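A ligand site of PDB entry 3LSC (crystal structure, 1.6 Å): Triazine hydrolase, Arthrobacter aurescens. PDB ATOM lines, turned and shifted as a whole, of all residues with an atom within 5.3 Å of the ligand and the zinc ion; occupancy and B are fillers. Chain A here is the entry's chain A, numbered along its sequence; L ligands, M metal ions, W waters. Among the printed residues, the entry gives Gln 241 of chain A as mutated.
A nitrogen (N4) of the ligand lies close to a ring nitrogen (NE2) of His 65, at 3.4 Å. N4 of the ligand lies close to OE2 of Glu 68 (3.1 Å). N1 of the ligand sits close to OE1 of Gln 241, 3.3 Å away.
A ring nitrogen (ND1) of His 238 sits at hydrogen-bond distance from the backbone carbonyl oxygen (O) of Cys 211. A ring nitrogen (ND1) of His 65 sits at hydrogen-bond distance from the backbone carbonyl oxygen (O) of Gln 129 (2.8 Å). The backbone carbonyl oxygen (O) of His 63 lies within hydrogen-bond range of the backbone NH (N) of Thr 325, 2.8 Å away. A ring nitrogen (NE2) of His 274 lies close to the side-chain amide oxygen of Gln 241, 3.4 Å away.
CE2 of Tyr 67 touches C5 of the ligand, 3.4 Å away. Met 82 touches the ligand (CE to N5, 3.6 Å). Trp 85 touches the ligand. Leu 86 touches the ligand. SG of Cys 211 touches C8 of the ligand, at 3.5 Å. Tyr 215 touches the ligand (CZ to C8, 3.2 Å). CE1 of His 274 touches C9 of the ligand (3.8 Å). Pro 299 touches the ligand. CH2 of Trp 305 touches C9 of the ligand, at 3.6 Å. Thr 325 touches the ligand (OG1 to O1, 3.98 Å). Ser 329 touches the ligand (OG to O1, 3.8 Å). Hydrophobic or aromatic side chains within 4 Å of the ligand: His 65, Tyr 67, Met 82, Trp 85, Leu 86, Tyr 215, His 238, His 274, Pro 299 and Trp 305. Within 4 Å of the ligand: His 65, Tyr 67, Glu 68, Met 82, Trp 85, Leu 86, Cys 211, Tyr 215, His 238, Gln 241, His 274, Pro 299, Trp 305, Thr 325 and Ser 329. The nearest printed residue that does not touch the ligand is Leu 131 (4.1 Å).
Residues that only touch the zinc ion: Thr 325 (3.4 Å). Four residues have an atom within 4 Å of the zinc ion: His 63, His 65, His 238 and Thr 325. The nearest printed residue that does not touch the zinc ion is Gln 129 (4.05 Å).
Water W1 is bound to the zinc ion. NE2 of His 238 binds the zinc ion (2.0 Å). A ring nitrogen (NE2) of His 65 is bound to the zinc ion, at 2.1 Å. NE2 of His 63 binds the zinc ion, 2.1 Å away. The zinc ion has four donor atoms within binding distance.
Water W1 lies within hydrogen-bond range of the side-chain hydroxyl (OG1) of Thr 325 (2.5 Å), a ring nitrogen (NE2) of His 274 (2.9 Å) and an oxygen (O1) of the ligand (3.1 Å). Water W2 lies within hydrogen-bond range of a nitrogen (N2) of the ligand (2.7 Å), the side-chain carboxylate of Glu 68 (2.7 Å) and the side-chain hydroxyl of Thr 325 (3.1 Å).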
ATOM      1  N   HIS A  63      25.535  -3.552 -27.956  1.00  0.00           N
ATOM      2  CA  HIS A  63      25.535  -4.748 -27.097  1.00  0.00           C
ATOM      3  C   HIS A  63      25.495  -4.398 -25.602  1.00  0.00           C
ATOM      4  O   HIS A  63      26.505  -3.960 -25.034  1.00  0.00           O
ATOM      5  CB  HIS A  63      26.751  -5.626 -27.420  1.00  0.00           C
ATOM      6  CG  HIS A  63      26.712  -6.995 -26.781  1.00  0.00           C
ATOM      7  ND1 HIS A  63      25.974  -8.034 -27.283  1.00  0.00           N
ATOM      8  CD2 HIS A  63      27.370  -7.479 -25.698  1.00  0.00           C
ATOM      9  CE1 HIS A  63      26.150  -9.111 -26.527  1.00  0.00           C
ATOM     10  NE2 HIS A  63      27.000  -8.799 -25.566  1.00  0.00           N
ATOM     11  N   HIS A  65      23.786  -5.809 -21.585  1.00  0.00           N
ATOM     12  CA  HIS A  65      23.041  -6.757 -20.750  1.00  0.00           C
ATOM     13  C   HIS A  65      22.551  -5.925 -19.564  1.00  0.00           C
ATOM     14  O   HIS A  65      23.216  -5.816 -18.522  1.00  0.00           O
ATOM     15  CB  HIS A  65      23.922  -7.892 -20.239  1.00  0.00           C
ATOM     16  CG  HIS A  65      24.583  -8.676 -21.336  1.00  0.00           C
ATOM     17  ND1 HIS A  65      23.867  -9.269 -22.349  1.00  0.00           N
ATOM     18  CD2 HIS A  65      25.883  -8.978 -21.558  1.00  0.00           C
ATOM     19  CE1 HIS A  65      24.695  -9.902 -23.163  1.00  0.00           C
ATOM     20  NE2 HIS A  65      25.925  -9.743 -22.703  1.00  0.00           N
ATOM     21  N   TYR A  67      20.313  -6.055 -17.232  1.00  0.00           N
ATOM     22  CA  TYR A  67      20.059  -6.569 -15.877  1.00  0.00           C
ATOM     23  C   TYR A  67      21.322  -6.630 -15.019  1.00  0.00           C
ATOM     24  O   TYR A  67      21.236  -6.654 -13.785  1.00  0.00           O
ATOM     25  CB  TYR A  67      19.320  -7.914 -15.918  1.00  0.00           C
ATOM     26  CG  TYR A  67      20.189  -9.129 -16.064  1.00  0.00           C
ATOM     27  CD1 TYR A  67      20.130 -10.167 -15.136  1.00  0.00           C
ATOM     28  CD2 TYR A  67      21.050  -9.278 -17.147  1.00  0.00           C
ATOM     29  CE1 TYR A  67      20.921 -11.288 -15.267  1.00  0.00           C
ATOM     30  CE2 TYR A  67      21.848 -10.407 -17.281  1.00  0.00           C
ATOM     31  CZ  TYR A  67      21.774 -11.407 -16.342  1.00  0.00           C
ATOM     32  OH  TYR A  67      22.548 -12.540 -16.449  1.00  0.00           O
ATOM     33  N   GLU A  68      22.489  -6.615 -15.649  1.00  0.00           N
ATOM     34  CA  GLU A  68      23.770  -6.587 -14.932  1.00  0.00           C
ATOM     35  C   GLU A  68      24.081  -5.269 -14.201  1.00  0.00           C
ATOM     36  O   GLU A  68      25.053  -5.178 -13.461  1.00  0.00           O
ATOM     37  CB  GLU A  68      24.929  -6.956 -15.854  1.00  0.00           C
ATOM     38  CG  GLU A  68      24.836  -8.367 -16.424  1.00  0.00           C
ATOM     39  CD  GLU A  68      26.002  -8.723 -17.330  1.00  0.00           C
ATOM     40  OE1 GLU A  68      26.926  -7.893 -17.482  1.00  0.00           O
ATOM     41  OE2 GLU A  68      25.976  -9.842 -17.876  1.00  0.00           O
ATOM     42  N   MET A  82      36.972 -15.787 -17.144  1.00  0.00           N
ATOM     43  CA  MET A  82      35.602 -15.962 -17.635  1.00  0.00           C
ATOM     44  C   MET A  82      34.785 -17.022 -16.896  1.00  0.00           C
ATOM     45  O   MET A  82      33.617 -16.786 -16.562  1.00  0.00           O
ATOM     46  CB  MET A  82      35.617 -16.275 -19.139  1.00  0.00           C
ATOM     47  CG  MET A  82      34.215 -16.479 -19.702  1.00  0.00           C
ATOM     48  SD  MET A  82      33.226 -15.007 -19.416  1.00  0.00           S
ATOM     49  CE  MET A  82      31.784 -15.390 -20.422  1.00  0.00           C
ATOM     50  N   TRP A  85      33.721 -15.931 -13.537  1.00  0.00           N
ATOM     51  CA  TRP A  85      32.817 -14.802 -13.705  1.00  0.00           C
ATOM     52  C   TRP A  85      31.413 -15.248 -14.067  1.00  0.00           C
ATOM     53  O   TRP A  85      30.442 -14.809 -13.446  1.00  0.00           O
ATOM     54  CB  TRP A  85      33.362 -13.865 -14.785  1.00  0.00           C
ATOM     55  CG  TRP A  85      32.519 -12.647 -14.999  1.00  0.00           C
ATOM     56  CD1 TRP A  85      32.658 -11.439 -14.386  1.00  0.00           C
ATOM     57  CD2 TRP A  85      31.416 -12.520 -15.901  1.00  0.00           C
ATOM     58  NE1 TRP A  85      31.696 -10.569 -14.846  1.00  0.00           N
ATOM     59  CE2 TRP A  85      30.922 -11.209 -15.774  1.00  0.00           C
ATOM     60  CE3 TRP A  85      30.790 -13.401 -16.810  1.00  0.00           C
ATOM     61  CZ2 TRP A  85      29.841 -10.738 -16.528  1.00  0.00           C
ATOM     62  CZ3 TRP A  85      29.709 -12.940 -17.543  1.00  0.00           C
ATOM     63  CH2 TRP A  85      29.247 -11.622 -17.393  1.00  0.00           C
ATOM     64  N   LEU A  86      31.319 -16.111 -15.069  1.00  0.00           N
ATOM     65  CA  LEU A  86      30.024 -16.554 -15.573  1.00  0.00           C
ATOM     66  C   LEU A  86      29.275 -17.324 -14.494  1.00  0.00           C
ATOM     67  O   LEU A  86      28.068 -17.112 -14.289  1.00  0.00           O
ATOM     68  CB  LEU A  86      30.202 -17.396 -16.847  1.00  0.00           C
ATOM     69  CG  LEU A  86      28.930 -17.748 -17.619  1.00  0.00           C
ATOM     70  CD1 LEU A  86      28.155 -16.494 -18.011  1.00  0.00           C
ATOM     71  CD2 LEU A  86      29.274 -18.581 -18.854  1.00  0.00           C
ATOM     72  N   VAL A  89      27.955 -14.771 -11.932  1.00  0.00           N
ATOM     73  CA  VAL A  89      26.828 -13.982 -12.394  1.00  0.00           C
ATOM     74  C   VAL A  89      25.543 -14.813 -12.420  1.00  0.00           C
ATOM     75  O   VAL A  89      24.481 -14.356 -11.975  1.00  0.00           O
ATOM     76  CB  VAL A  89      27.099 -13.383 -13.780  1.00  0.00           C
ATOM     77  CG1 VAL A  89      25.827 -12.785 -14.375  1.00  0.00           C
ATOM     78  CG2 VAL A  89      28.188 -12.329 -13.700  1.00  0.00           C
ATOM     79  N   LEU A  90      25.652 -16.036 -12.929  1.00  0.00           N
ATOM     80  CA  LEU A  90      24.490 -16.929 -13.047  1.00  0.00           C
ATOM     81  C   LEU A  90      24.001 -17.367 -11.676  1.00  0.00           C
ATOM     82  O   LEU A  90      22.788 -17.408 -11.426  1.00  0.00           O
ATOM     83  CB  LEU A  90      24.829 -18.149 -13.911  1.00  0.00           C
ATOM     84  CG  LEU A  90      25.121 -17.835 -15.383  1.00  0.00           C
ATOM     85  CD1 LEU A  90      25.524 -19.099 -16.137  1.00  0.00           C
ATOM     86  CD2 LEU A  90      23.910 -17.169 -16.044  1.00  0.00           C
ATOM     87  N   GLN A 129      20.638  -7.595 -24.772  1.00  0.00           N
ATOM     88  CA  GLN A 129      20.521  -9.041 -24.937  1.00  0.00           C
ATOM     89  C   GLN A 129      20.256  -9.668 -23.574  1.00  0.00           C
ATOM     90  O   GLN A 129      21.170  -9.811 -22.744  1.00  0.00           O
ATOM     91  CB  GLN A 129      21.789  -9.612 -25.578  1.00  0.00           C
ATOM     92  CG  GLN A 129      21.697 -11.100 -25.928  1.00  0.00           C
ATOM     93  CD  GLN A 129      23.013 -11.665 -26.408  1.00  0.00           C
ATOM     94  OE1 GLN A 129      24.088 -11.258 -25.965  1.00  0.00           O
ATOM     95  NE2 GLN A 129      22.941 -12.623 -27.339  1.00  0.00           N
ATOM     96  N   LEU A 131      19.049 -12.846 -21.408  1.00  0.00           N
ATOM     97  CA  LEU A 131      18.897 -14.311 -21.436  1.00  0.00           C
ATOM     98  C   LEU A 131      18.284 -14.909 -20.158  1.00  0.00           C
ATOM     99  O   LEU A 131      18.002 -16.110 -20.117  1.00  0.00           O
ATOM    100  CB  LEU A 131      20.239 -14.991 -21.717  1.00  0.00           C
ATOM    101  CG  LEU A 131      21.385 -14.778 -20.717  1.00  0.00           C
ATOM    102  CD1 LEU A 131      21.069 -15.454 -19.382  1.00  0.00           C
ATOM    103  CD2 LEU A 131      22.680 -15.323 -21.292  1.00  0.00           C
ATOM    104  N   CYS A 211      22.688 -16.917 -26.805  1.00  0.00           N
ATOM    105  CA  CYS A 211      23.888 -16.531 -26.069  1.00  0.00           C
ATOM    106  C   CYS A 211      25.144 -16.907 -26.859  1.00  0.00           C
ATOM    107  O   CYS A 211      26.089 -16.129 -26.945  1.00  0.00           O
ATOM    108  CB  CYS A 211      23.895 -17.169 -24.688  1.00  0.00           C
ATOM    109  SG  CYS A 211      25.176 -16.435 -23.653  1.00  0.00           S
ATOM    110  N   TYR A 215      26.505 -22.315 -25.884  1.00  0.00           N
ATOM    111  CA  TYR A 215      25.415 -22.164 -24.934  1.00  0.00           C
ATOM    112  C   TYR A 215      24.043 -22.525 -25.463  1.00  0.00           C
ATOM    113  O   TYR A 215      23.082 -22.590 -24.699  1.00  0.00           O
ATOM    114  CB  TYR A 215      25.359 -20.720 -24.428  1.00  0.00           C
ATOM    115  CG  TYR A 215      26.684 -20.207 -23.960  1.00  0.00           C
ATOM    116  CD1 TYR A 215      27.225 -20.624 -22.749  1.00  0.00           C
ATOM    117  CD2 TYR A 215      27.422 -19.322 -24.725  1.00  0.00           C
ATOM    118  CE1 TYR A 215      28.435 -20.165 -22.303  1.00  0.00           C
ATOM    119  CE2 TYR A 215      28.646 -18.857 -24.296  1.00  0.00           C
ATOM    120  CZ  TYR A 215      29.154 -19.280 -23.078  1.00  0.00           C
ATOM    121  OH  TYR A 215      30.374 -18.822 -22.643  1.00  0.00           O
ATOM    122  N   HIS A 238      27.108 -13.887 -29.361  1.00  0.00           N
ATOM    123  CA  HIS A 238      28.516 -13.727 -29.023  1.00  0.00           C
ATOM    124  C   HIS A 238      29.396 -14.493 -30.017  1.00  0.00           C
ATOM    125  O   HIS A 238      28.958 -15.474 -30.611  1.00  0.00           O
ATOM    126  CB  HIS A 238      28.792 -14.205 -27.602  1.00  0.00           C
ATOM    127  CG  HIS A 238      28.124 -13.383 -26.547  1.00  0.00           C
ATOM    128  ND1 HIS A 238      26.970 -13.785 -25.914  1.00  0.00           N
ATOM    129  CD2 HIS A 238      28.454 -12.175 -26.021  1.00  0.00           C
ATOM    130  CE1 HIS A 238      26.618 -12.871 -25.029  1.00  0.00           C
ATOM    131  NE2 HIS A 238      27.495 -11.886 -25.080  1.00  0.00           N
ATOM    132  N   GLN A 241      34.847 -15.441 -28.385  1.00  0.00           N
ATOM    133  CA  GLN A 241      35.455 -15.223 -27.085  1.00  0.00           C
ATOM    134  C   GLN A 241      36.499 -16.338 -26.946  1.00  0.00           C
ATOM    135  O   GLN A 241      36.313 -17.430 -27.466  1.00  0.00           O
ATOM    136  CB  GLN A 241      34.408 -15.310 -25.981  1.00  0.00           C
ATOM    137  CG  GLN A 241      33.274 -14.286 -26.133  1.00  0.00           C
ATOM    138  CD  GLN A 241      32.378 -14.189 -24.898  1.00  0.00           C
ATOM    139  OE1 GLN A 241      31.799 -13.134 -24.614  1.00  0.00           O
ATOM    140  NE2 GLN A 241      32.280 -15.284 -24.158  1.00  0.00           N
ATOM    141  N   ALA A 273      28.993 -10.136 -31.404  1.00  0.00           N
ATOM    142  CA  ALA A 273      29.622  -9.406 -30.298  1.00  0.00           C
ATOM    143  C   ALA A 273      31.024  -9.924 -29.982  1.00  0.00           C
ATOM    144  O   ALA A 273      31.242 -11.139 -29.893  1.00  0.00           O
ATOM    145  CB  ALA A 273      28.726  -9.515 -29.047  1.00  0.00           C
ATOM    146  N   HIS A 274      31.970  -8.992 -29.785  1.00  0.00           N
ATOM    147  CA  HIS A 274      33.373  -9.271 -29.426  1.00  0.00           C
ATOM    148  C   HIS A 274      34.273  -9.610 -30.617  1.00  0.00           C
ATOM    149  O   HIS A 274      35.110  -8.800 -31.020  1.00  0.00           O
ATOM    150  CB  HIS A 274      33.503 -10.362 -28.360  1.00  0.00           C
ATOM    151  CG  HIS A 274      32.807 -10.063 -27.068  1.00  0.00           C
ATOM    152  ND1 HIS A 274      33.357  -9.252 -26.090  1.00  0.00           N
ATOM    153  CD2 HIS A 274      31.593 -10.437 -26.600  1.00  0.00           C
ATOM    154  CE1 HIS A 274      32.530  -9.174 -25.067  1.00  0.00           C
ATOM    155  NE2 HIS A 274      31.440  -9.871 -25.360  1.00  0.00           N
ATOM    156  N   PRO A 299      35.021  -5.117 -21.857  1.00  0.00           N
ATOM    157  CA  PRO A 299      35.017  -6.506 -21.362  1.00  0.00           C
ATOM    158  C   PRO A 299      36.208  -7.333 -21.899  1.00  0.00           C
ATOM    159  O   PRO A 299      36.731  -8.192 -21.168  1.00  0.00           O
ATOM    160  CB  PRO A 299      33.698  -7.070 -21.901  1.00  0.00           C
ATOM    161  CG  PRO A 299      33.291  -6.182 -23.022  1.00  0.00           C
ATOM    162  CD  PRO A 299      33.826  -4.805 -22.655  1.00  0.00           C
ATOM    163  N   MET A 303      38.446  -9.122 -19.033  1.00  0.00           N
ATOM    164  CA  MET A 303      38.535 -10.582 -18.915  1.00  0.00           C
ATOM    165  C   MET A 303      39.933 -11.096 -19.233  1.00  0.00           C
ATOM    166  O   MET A 303      40.184 -12.305 -19.120  1.00  0.00           O
ATOM    167  CB  MET A 303      37.508 -11.263 -19.825  1.00  0.00           C
ATOM    168  CG  MET A 303      36.090 -10.924 -19.472  1.00  0.00           C
ATOM    169  SD  MET A 303      35.688 -11.635 -17.867  1.00  0.00           S
ATOM    170  CE  MET A 303      35.008 -10.197 -17.088  1.00  0.00           C
ATOM    171  N   TRP A 305      41.266 -10.898 -22.228  1.00  0.00           N
ATOM    172  CA  TRP A 305      41.198 -11.500 -23.559  1.00  0.00           C
ATOM    173  C   TRP A 305      42.114 -10.823 -24.562  1.00  0.00           C
ATOM    174  O   TRP A 305      42.698 -11.466 -25.413  1.00  0.00           O
ATOM    175  CB  TRP A 305      39.760 -11.458 -24.077  1.00  0.00           C
ATOM    176  CG  TRP A 305      38.844 -12.350 -23.311  1.00  0.00           C
ATOM    177  CD1 TRP A 305      39.198 -13.345 -22.460  1.00  0.00           C
ATOM    178  CD2 TRP A 305      37.414 -12.342 -23.351  1.00  0.00           C
ATOM    179  NE1 TRP A 305      38.083 -13.957 -21.952  1.00  0.00           N
ATOM    180  CE2 TRP A 305      36.967 -13.359 -22.479  1.00  0.00           C
ATOM    181  CE3 TRP A 305      36.463 -11.572 -24.026  1.00  0.00           C
ATOM    182  CZ2 TRP A 305      35.620 -13.630 -22.277  1.00  0.00           C
ATOM    183  CZ3 TRP A 305      35.127 -11.834 -23.825  1.00  0.00           C
ATOM    184  CH2 TRP A 305      34.712 -12.865 -22.949  1.00  0.00           C
ATOM    185  N   THR A 325      28.908  -3.937 -23.528  1.00  0.00           N
ATOM    186  CA  THR A 325      28.424  -5.105 -22.783  1.00  0.00           C
ATOM    187  C   THR A 325      27.748  -4.692 -21.480  1.00  0.00           C
ATOM    188  O   THR A 325      27.614  -3.502 -21.186  1.00  0.00           O
ATOM    189  CB  THR A 325      29.490  -6.241 -22.580  1.00  0.00           C
ATOM    190  OG1 THR A 325      28.786  -7.483 -22.452  1.00  0.00           O
ATOM    191  CG2 THR A 325      30.325  -6.039 -21.320  1.00  0.00           C
ATOM    192  N   SER A 329      30.565  -6.730 -16.393  1.00  0.00           N
ATOM    193  CA  SER A 329      31.867  -6.892 -17.052  1.00  0.00           C
ATOM    194  C   SER A 329      32.245  -5.598 -17.754  1.00  0.00           C
ATOM    195  O   SER A 329      32.609  -5.611 -18.933  1.00  0.00           O
ATOM    196  CB  SER A 329      31.830  -8.036 -18.074  1.00  0.00           C
ATOM    197  OG  SER A 329      33.118  -8.200 -18.657  1.00  0.00           O
HETATM  198  N1  LIG L   1      30.237 -12.348 -21.865  1.00  0.00           N
HETATM  199  C1  LIG L   1      30.052 -11.276 -21.126  1.00  0.00           C
HETATM  200  N2  LIG L   1      28.857 -11.034 -20.526  1.00  0.00           N
HETATM  201  C2  LIG L   1      27.848 -11.948 -20.697  1.00  0.00           C
HETATM  202  N3  LIG L   1      28.039 -13.047 -21.428  1.00  0.00           N
HETATM  203  C3  LIG L   1      29.184 -13.267 -22.020  1.00  0.00           C
HETATM  204  N4  LIG L   1      26.561 -11.876 -20.097  1.00  0.00           N
HETATM  205  C4  LIG L   1      25.345 -12.564 -19.768  1.00  0.00           C
HETATM  206  C5  LIG L   1      24.165 -11.714 -19.436  1.00  0.00           C
HETATM  207  C6  LIG L   1      25.617 -13.686 -18.828  1.00  0.00           C
HETATM  208  N5  LIG L   1      29.268 -14.469 -22.771  1.00  0.00           N
HETATM  209  C7  LIG L   1      28.858 -15.801 -23.076  1.00  0.00           C
HETATM  210  C8  LIG L   1      28.243 -16.484 -21.904  1.00  0.00           C
HETATM  211  O1  LIG L   1      31.088 -10.370 -20.977  1.00  0.00           O
HETATM  212  C9  LIG L   1      32.302 -10.633 -21.586  1.00  0.00           C
HETATM  213 ZN    ZN M   1      27.462 -10.137 -24.026  1.00  0.00          ZN
HETATM  214  O   HOH W   1      29.320  -9.776 -23.414  1.00  0.00           O
HETATM  215  O   HOH W   2      28.601  -8.500 -19.561  1.00  0.00           O
